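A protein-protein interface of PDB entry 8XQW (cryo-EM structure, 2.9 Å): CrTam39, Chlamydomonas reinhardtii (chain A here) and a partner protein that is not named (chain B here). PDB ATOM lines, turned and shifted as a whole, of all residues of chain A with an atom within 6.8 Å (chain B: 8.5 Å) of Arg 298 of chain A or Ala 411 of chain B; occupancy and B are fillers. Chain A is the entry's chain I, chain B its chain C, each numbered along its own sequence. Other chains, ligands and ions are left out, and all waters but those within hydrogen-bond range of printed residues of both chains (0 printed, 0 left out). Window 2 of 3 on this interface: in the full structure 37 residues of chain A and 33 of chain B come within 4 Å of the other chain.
O of Ala 411 of chain B is in hydrogen-bond range of NH2 of Arg 298 of chain A, 2.8 Å away.
The backbone carbonyl oxygen (O) of Arg 298 of chain A sits at hydrogen-bond distance from the backbone NH (N) of Glu 415 of chain B (3.1 Å).
The backbone carbonyl oxygen (O) of Ala 409 of chain B lies within hydrogen-bond range of the guanidinium group (NE) of Arg 298 of chain A, 3.2 Å away.
Among the printed residues, merely in contact across the chains: Arg 298 of chain A with Gly 413 of chain B (3.8 Å), Arg 298 of chain A with Gly 414 of chain B (3.5 Å), Arg 299 of chain A with Ala 409 of chain B (3.3 Å) and Leu 300 of chain A with Glu 415 of chain B (3.3 Å).
Of the printed residues of chain A, Ala 411 of chain B touches Arg 298.
Of the printed residues of chain A, Ala 409 of chain B touches Arg 298 (3.2 Å) and Arg 299 (3.3 Å).
Of the printed residues of chain A, Gly 414 of chain B touches Arg 298.
Of the printed residues of chain A, Glu 415 of chain B touches Arg 298 (3.1 Å) and Leu 300 (3.3 Å).
Hydrophobic or aromatic side chains of chain B within 4 Å of the printed part of chain A: Ala 409.
Among the printed residues, 7 pairs touch across the chains.
Among the printed residues, no Asp or Glu carboxylate lies within 4 Å of a Lys or Arg side-chain nitrogen of the other chain.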
ATOM      1  N   ARG A 296     -28.116 -22.899  -7.025  1.00  0.00           N
ATOM      2  CA  ARG A 296     -27.818 -21.523  -7.369  1.00  0.00           C
ATOM      3  C   ARG A 296     -28.091 -21.282  -8.845  1.00  0.00           C
ATOM      4  O   ARG A 296     -27.908 -22.168  -9.682  1.00  0.00           O
ATOM      5  CB  ARG A 296     -26.363 -21.197  -7.070  1.00  0.00           C
ATOM      6  CG  ARG A 296     -25.982 -21.253  -5.626  1.00  0.00           C
ATOM      7  CD  ARG A 296     -24.505 -20.976  -5.501  1.00  0.00           C
ATOM      8  NE  ARG A 296     -24.114 -20.655  -4.137  1.00  0.00           N
ATOM      9  CZ  ARG A 296     -24.266 -19.460  -3.581  1.00  0.00           C
ATOM     10  NH1 ARG A 296     -23.881 -19.258  -2.330  1.00  0.00           N
ATOM     11  NH2 ARG A 296     -24.807 -18.469  -4.272  1.00  0.00           N
ATOM     12  N   LYS A 297     -28.522 -20.072  -9.160  1.00  0.00           N
ATOM     13  CA  LYS A 297     -28.773 -19.654 -10.528  1.00  0.00           C
ATOM     14  C   LYS A 297     -27.934 -18.423 -10.846  1.00  0.00           C
ATOM     15  O   LYS A 297     -27.100 -17.987 -10.052  1.00  0.00           O
ATOM     16  CB  LYS A 297     -30.259 -19.374 -10.752  1.00  0.00           C
ATOM     17  CG  LYS A 297     -31.167 -20.474 -10.269  1.00  0.00           C
ATOM     18  CD  LYS A 297     -30.787 -21.797 -10.899  1.00  0.00           C
ATOM     19  CE  LYS A 297     -32.004 -22.561 -11.375  1.00  0.00           C
ATOM     20  NZ  LYS A 297     -31.909 -24.003 -11.025  1.00  0.00           N
ATOM     21  N   ARG A 298     -28.159 -17.862 -12.034  1.00  0.00           N
ATOM     22  CA  ARG A 298     -27.457 -16.645 -12.417  1.00  0.00           C
ATOM     23  C   ARG A 298     -28.108 -15.413 -11.808  1.00  0.00           C
ATOM     24  O   ARG A 298     -27.411 -14.506 -11.347  1.00  0.00           O
ATOM     25  CB  ARG A 298     -27.411 -16.522 -13.937  1.00  0.00           C
ATOM     26  CG  ARG A 298     -26.757 -17.690 -14.633  1.00  0.00           C
ATOM     27  CD  ARG A 298     -25.961 -17.217 -15.827  1.00  0.00           C
ATOM     28  NE  ARG A 298     -24.696 -16.619 -15.418  1.00  0.00           N
ATOM     29  CZ  ARG A 298     -23.573 -17.302 -15.242  1.00  0.00           C
ATOM     30  NH1 ARG A 298     -23.554 -18.609 -15.448  1.00  0.00           N
ATOM     31  NH2 ARG A 298     -22.466 -16.681 -14.867  1.00  0.00           N
ATOM     32  N   ARG A 299     -29.434 -15.375 -11.781  1.00  0.00           N
ATOM     33  CA  ARG A 299     -30.154 -14.238 -11.234  1.00  0.00           C
ATOM     34  C   ARG A 299     -30.023 -14.209  -9.714  1.00  0.00           C
ATOM     35  O   ARG A 299     -29.262 -14.964  -9.109  1.00  0.00           O
ATOM     36  CB  ARG A 299     -31.619 -14.298 -11.642  1.00  0.00           C
ATOM     37  CG  ARG A 299     -31.831 -14.329 -13.132  1.00  0.00           C
ATOM     38  CD  ARG A 299     -31.681 -12.946 -13.732  1.00  0.00           C
ATOM     39  NE  ARG A 299     -32.297 -12.877 -15.051  1.00  0.00           N
ATOM     40  CZ  ARG A 299     -31.638 -13.064 -16.187  1.00  0.00           C
ATOM     41  NH1 ARG A 299     -32.275 -12.988 -17.346  1.00  0.00           N
ATOM     42  NH2 ARG A 299     -30.342 -13.325 -16.166  1.00  0.00           N
ATOM     43  N   LEU A 300     -30.766 -13.304  -9.088  1.00  0.00           N
ATOM     44  CA  LEU A 300     -30.793 -13.205  -7.637  1.00  0.00           C
ATOM     45  C   LEU A 300     -32.111 -13.642  -7.029  1.00  0.00           C
ATOM     46  O   LEU A 300     -32.118 -14.216  -5.943  1.00  0.00           O
ATOM     47  CB  LEU A 300     -30.493 -11.776  -7.189  1.00  0.00           C
ATOM     48  CG  LEU A 300     -29.226 -11.604  -6.356  1.00  0.00           C
ATOM     49  CD1 LEU A 300     -29.271 -10.300  -5.587  1.00  0.00           C
ATOM     50  CD2 LEU A 300     -29.048 -12.778  -5.419  1.00  0.00           C
ATOM     51  N   ALA A 302     -34.058 -15.705  -8.754  1.00  0.00           N
ATOM     52  CA  ALA A 302     -34.211 -17.071  -9.227  1.00  0.00           C
ATOM     53  C   ALA A 302     -33.566 -18.068  -8.280  1.00  0.00           C
ATOM     54  O   ALA A 302     -33.967 -19.235  -8.246  1.00  0.00           O
ATOM     55  CB  ALA A 302     -33.613 -17.213 -10.625  1.00  0.00           C
ATOM     56  N   SER A 303     -32.570 -17.629  -7.510  1.00  0.00           N
ATOM     57  CA  SER A 303     -31.876 -18.473  -6.550  1.00  0.00           C
ATOM     58  C   SER A 303     -32.265 -18.154  -5.114  1.00  0.00           C
ATOM     59  O   SER A 303     -31.408 -18.154  -4.228  1.00  0.00           O
ATOM     60  CB  SER A 303     -30.368 -18.336  -6.725  1.00  0.00           C
ATOM     61  OG  SER A 303     -29.833 -17.482  -5.739  1.00  0.00           O
ATOM     62  N   LEU B 384     -13.615  -5.216 -13.317  1.00  0.00           N
ATOM     63  CA  LEU B 384     -14.985  -5.681 -13.484  1.00  0.00           C
ATOM     64  C   LEU B 384     -15.866  -4.591 -14.063  1.00  0.00           C
ATOM     65  O   LEU B 384     -16.689  -4.854 -14.947  1.00  0.00           O
ATOM     66  CB  LEU B 384     -15.533  -6.155 -12.145  1.00  0.00           C
ATOM     67  CG  LEU B 384     -15.448  -7.652 -11.898  1.00  0.00           C
ATOM     68  CD1 LEU B 384     -15.402  -7.930 -10.414  1.00  0.00           C
ATOM     69  CD2 LEU B 384     -16.632  -8.341 -12.534  1.00  0.00           C
ATOM     70  N   GLU B 387     -14.892  -4.351 -17.758  1.00  0.00           N
ATOM     71  CA  GLU B 387     -15.455  -5.371 -18.631  1.00  0.00           C
ATOM     72  C   GLU B 387     -16.969  -5.275 -18.749  1.00  0.00           C
ATOM     73  O   GLU B 387     -17.578  -6.139 -19.385  1.00  0.00           O
ATOM     74  CB  GLU B 387     -15.049  -6.765 -18.149  1.00  0.00           C
ATOM     75  CG  GLU B 387     -15.789  -7.257 -16.923  1.00  0.00           C
ATOM     76  CD  GLU B 387     -15.359  -8.654 -16.504  1.00  0.00           C
ATOM     77  OE1 GLU B 387     -14.962  -8.834 -15.334  1.00  0.00           O
ATOM     78  OE2 GLU B 387     -15.427  -9.574 -17.342  1.00  0.00           O
ATOM     79  N   GLY B 388     -17.583  -4.251 -18.166  1.00  0.00           N
ATOM     80  CA  GLY B 388     -19.008  -4.044 -18.304  1.00  0.00           C
ATOM     81  C   GLY B 388     -19.863  -4.914 -17.420  1.00  0.00           C
ATOM     82  O   GLY B 388     -21.040  -5.121 -17.736  1.00  0.00           O
ATOM     83  N   HIS B 389     -19.318  -5.421 -16.317  1.00  0.00           N
ATOM     84  CA  HIS B 389     -20.028  -6.399 -15.511  1.00  0.00           C
ATOM     85  C   HIS B 389     -20.723  -5.810 -14.296  1.00  0.00           C
ATOM     86  O   HIS B 389     -21.799  -6.291 -13.933  1.00  0.00           O
ATOM     87  CB  HIS B 389     -19.070  -7.504 -15.071  1.00  0.00           C
ATOM     88  CG  HIS B 389     -18.948  -8.609 -16.070  1.00  0.00           C
ATOM     89  ND1 HIS B 389     -19.683  -8.635 -17.236  1.00  0.00           N
ATOM     90  CD2 HIS B 389     -18.197  -9.733 -16.075  1.00  0.00           C
ATOM     91  CE1 HIS B 389     -19.379  -9.721 -17.921  1.00  0.00           C
ATOM     92  NE2 HIS B 389     -18.478 -10.404 -17.239  1.00  0.00           N
ATOM     93  N   VAL B 390     -20.154  -4.788 -13.663  1.00  0.00           N
ATOM     94  CA  VAL B 390     -20.845  -4.128 -12.566  1.00  0.00           C
ATOM     95  C   VAL B 390     -22.098  -3.461 -13.107  1.00  0.00           C
ATOM     96  O   VAL B 390     -22.075  -2.847 -14.179  1.00  0.00           O
ATOM     97  CB  VAL B 390     -19.924  -3.118 -11.880  1.00  0.00           C
ATOM     98  CG1 VAL B 390     -20.671  -2.397 -10.790  1.00  0.00           C
ATOM     99  CG2 VAL B 390     -18.713  -3.817 -11.315  1.00  0.00           C
ATOM    100  N   ALA B 391     -23.202  -3.593 -12.386  1.00  0.00           N
ATOM    101  CA  ALA B 391     -24.489  -3.119 -12.871  1.00  0.00           C
ATOM    102  C   ALA B 391     -25.040  -1.946 -12.087  1.00  0.00           C
ATOM    103  O   ALA B 391     -25.776  -1.136 -12.647  1.00  0.00           O
ATOM    104  CB  ALA B 391     -25.516  -4.254 -12.848  1.00  0.00           C
ATOM    105  N   THR B 406     -23.451  -4.054  -7.004  1.00  0.00           N
ATOM    106  CA  THR B 406     -24.225  -5.211  -7.423  1.00  0.00           C
ATOM    107  C   THR B 406     -23.961  -5.475  -8.894  1.00  0.00           C
ATOM    108  O   THR B 406     -24.199  -4.606  -9.742  1.00  0.00           O
ATOM    109  CB  THR B 406     -25.718  -5.014  -7.164  1.00  0.00           C
ATOM    110  OG1 THR B 406     -26.475  -5.858  -8.037  1.00  0.00           O
ATOM    111  CG2 THR B 406     -26.112  -3.583  -7.362  1.00  0.00           C
ATOM    112  N   THR B 407     -23.472  -6.677  -9.181  1.00  0.00           N
ATOM    113  CA  THR B 407     -23.078  -7.108 -10.507  1.00  0.00           C
ATOM    114  C   THR B 407     -24.310  -7.495 -11.317  1.00  0.00           C
ATOM    115  O   THR B 407     -25.446  -7.384 -10.856  1.00  0.00           O
ATOM    116  CB  THR B 407     -22.096  -8.269 -10.396  1.00  0.00           C
ATOM    117  OG1 THR B 407     -21.343  -8.135  -9.191  1.00  0.00           O
ATOM    118  CG2 THR B 407     -21.129  -8.243 -11.535  1.00  0.00           C
ATOM    119  N   ARG B 408     -24.089  -7.947 -12.544  1.00  0.00           N
ATOM    120  CA  ARG B 408     -25.157  -8.398 -13.419  1.00  0.00           C
ATOM    121  C   ARG B 408     -24.972  -9.878 -13.725  1.00  0.00           C
ATOM    122  O   ARG B 408     -23.895 -10.447 -13.527  1.00  0.00           O
ATOM    123  CB  ARG B 408     -25.201  -7.580 -14.714  1.00  0.00           C
ATOM    124  CG  ARG B 408     -23.991  -7.746 -15.610  1.00  0.00           C
ATOM    125  CD  ARG B 408     -23.741  -6.491 -16.426  1.00  0.00           C
ATOM    126  NE  ARG B 408     -24.932  -5.651 -16.501  1.00  0.00           N
ATOM    127  CZ  ARG B 408     -24.912  -4.336 -16.695  1.00  0.00           C
ATOM    128  NH1 ARG B 408     -26.047  -3.654 -16.745  1.00  0.00           N
ATOM    129  NH2 ARG B 408     -23.759  -3.701 -16.844  1.00  0.00           N
ATOM    130  N   ALA B 409     -26.048 -10.496 -14.220  1.00  0.00           N
ATOM    131  CA  ALA B 409     -26.075 -11.945 -14.386  1.00  0.00           C
ATOM    132  C   ALA B 409     -24.940 -12.438 -15.271  1.00  0.00           C
ATOM    133  O   ALA B 409     -24.374 -13.509 -15.030  1.00  0.00           O
ATOM    134  CB  ALA B 409     -27.422 -12.377 -14.959  1.00  0.00           C
ATOM    135  N   SER B 410     -24.586 -11.669 -16.298  1.00  0.00           N
ATOM    136  CA  SER B 410     -23.588 -12.108 -17.265  1.00  0.00           C
ATOM    137  C   SER B 410     -22.213 -12.328 -16.651  1.00  0.00           C
ATOM    138  O   SER B 410     -21.372 -12.979 -17.280  1.00  0.00           O
ATOM    139  CB  SER B 410     -23.488 -11.085 -18.394  1.00  0.00           C
ATOM    140  OG  SER B 410     -24.758 -10.524 -18.675  1.00  0.00           O
ATOM    141  N   ALA B 411     -21.963 -11.818 -15.461  1.00  0.00           N
ATOM    142  CA  ALA B 411     -20.637 -11.907 -14.877  1.00  0.00           C
ATOM    143  C   ALA B 411     -20.312 -13.344 -14.482  1.00  0.00           C
ATOM    144  O   ALA B 411     -21.212 -14.176 -14.347  1.00  0.00           O
ATOM    145  CB  ALA B 411     -20.541 -11.006 -13.655  1.00  0.00           C
ATOM    146  N   PRO B 412     -19.028 -13.667 -14.301  1.00  0.00           N
ATOM    147  CA  PRO B 412     -18.680 -15.000 -13.795  1.00  0.00           C
ATOM    148  C   PRO B 412     -18.999 -15.127 -12.317  1.00  0.00           C
ATOM    149  O   PRO B 412     -18.250 -14.630 -11.471  1.00  0.00           O
ATOM    150  CB  PRO B 412     -17.171 -15.099 -14.052  1.00  0.00           C
ATOM    151  CG  PRO B 412     -16.811 -13.904 -14.878  1.00  0.00           C
ATOM    152  CD  PRO B 412     -17.832 -12.869 -14.599  1.00  0.00           C
ATOM    153  N   GLY B 413     -20.097 -15.800 -11.993  1.00  0.00           N
ATOM    154  CA  GLY B 413     -20.563 -15.928 -10.627  1.00  0.00           C
ATOM    155  C   GLY B 413     -21.959 -15.401 -10.391  1.00  0.00           C
ATOM    156  O   GLY B 413     -22.478 -15.537  -9.277  1.00  0.00           O
ATOM    157  N   GLY B 414     -22.587 -14.798 -11.395  1.00  0.00           N
ATOM    158  CA  GLY B 414     -23.943 -14.314 -11.253  1.00  0.00           C
ATOM    159  C   GLY B 414     -24.012 -13.044 -10.437  1.00  0.00           C
ATOM    160  O   GLY B 414     -23.006 -12.466 -10.031  1.00  0.00           O
ATOM    161  N   GLU B 415     -25.239 -12.602 -10.190  1.00  0.00           N
ATOM    162  CA  GLU B 415     -25.461 -11.394  -9.406  1.00  0.00           C
ATOM    163  C   GLU B 415     -25.009 -11.623  -7.976  1.00  0.00           C
ATOM    164  O   GLU B 415     -25.545 -12.488  -7.280  1.00  0.00           O
ATOM    165  CB  GLU B 415     -26.931 -11.001  -9.441  1.00  0.00           C
ATOM    166  CG  GLU B 415     -27.540 -11.040 -10.808  1.00  0.00           C
ATOM    167  CD  GLU B 415     -28.820 -10.254 -10.873  1.00  0.00           C
ATOM    168  OE1 GLU B 415     -29.219  -9.854 -11.986  1.00  0.00           O
ATOM    169  OE2 GLU B 415     -29.427 -10.028  -9.807  1.00  0.00           O
ATOM    170  N   ARG B 416     -24.026 -10.853  -7.530  1.00  0.00           N
ATOM    171  CA  ARG B 416     -23.609 -10.860  -6.142  1.00  0.00           C
ATOM    172  C   ARG B 416     -23.562  -9.428  -5.641  1.00  0.00           C
ATOM    173  O   ARG B 416     -23.757  -8.478  -6.396  1.00  0.00           O
ATOM    174  CB  ARG B 416     -22.250 -11.538  -5.964  1.00  0.00           C
ATOM    175  CG  ARG B 416     -21.453 -11.646  -7.235  1.00  0.00           C
ATOM    176  CD  ARG B 416     -20.258 -12.565  -7.048  1.00  0.00           C
ATOM    177  NE  ARG B 416     -19.557 -12.805  -8.306  1.00  0.00           N
ATOM    178  CZ  ARG B 416     -18.488 -12.125  -8.709  1.00  0.00           C
ATOM    179  NH1 ARG B 416     -17.917 -12.414  -9.869  1.00  0.00           N
ATOM    180  NH2 ARG B 416     -17.992 -11.156  -7.953  1.00  0.00           N
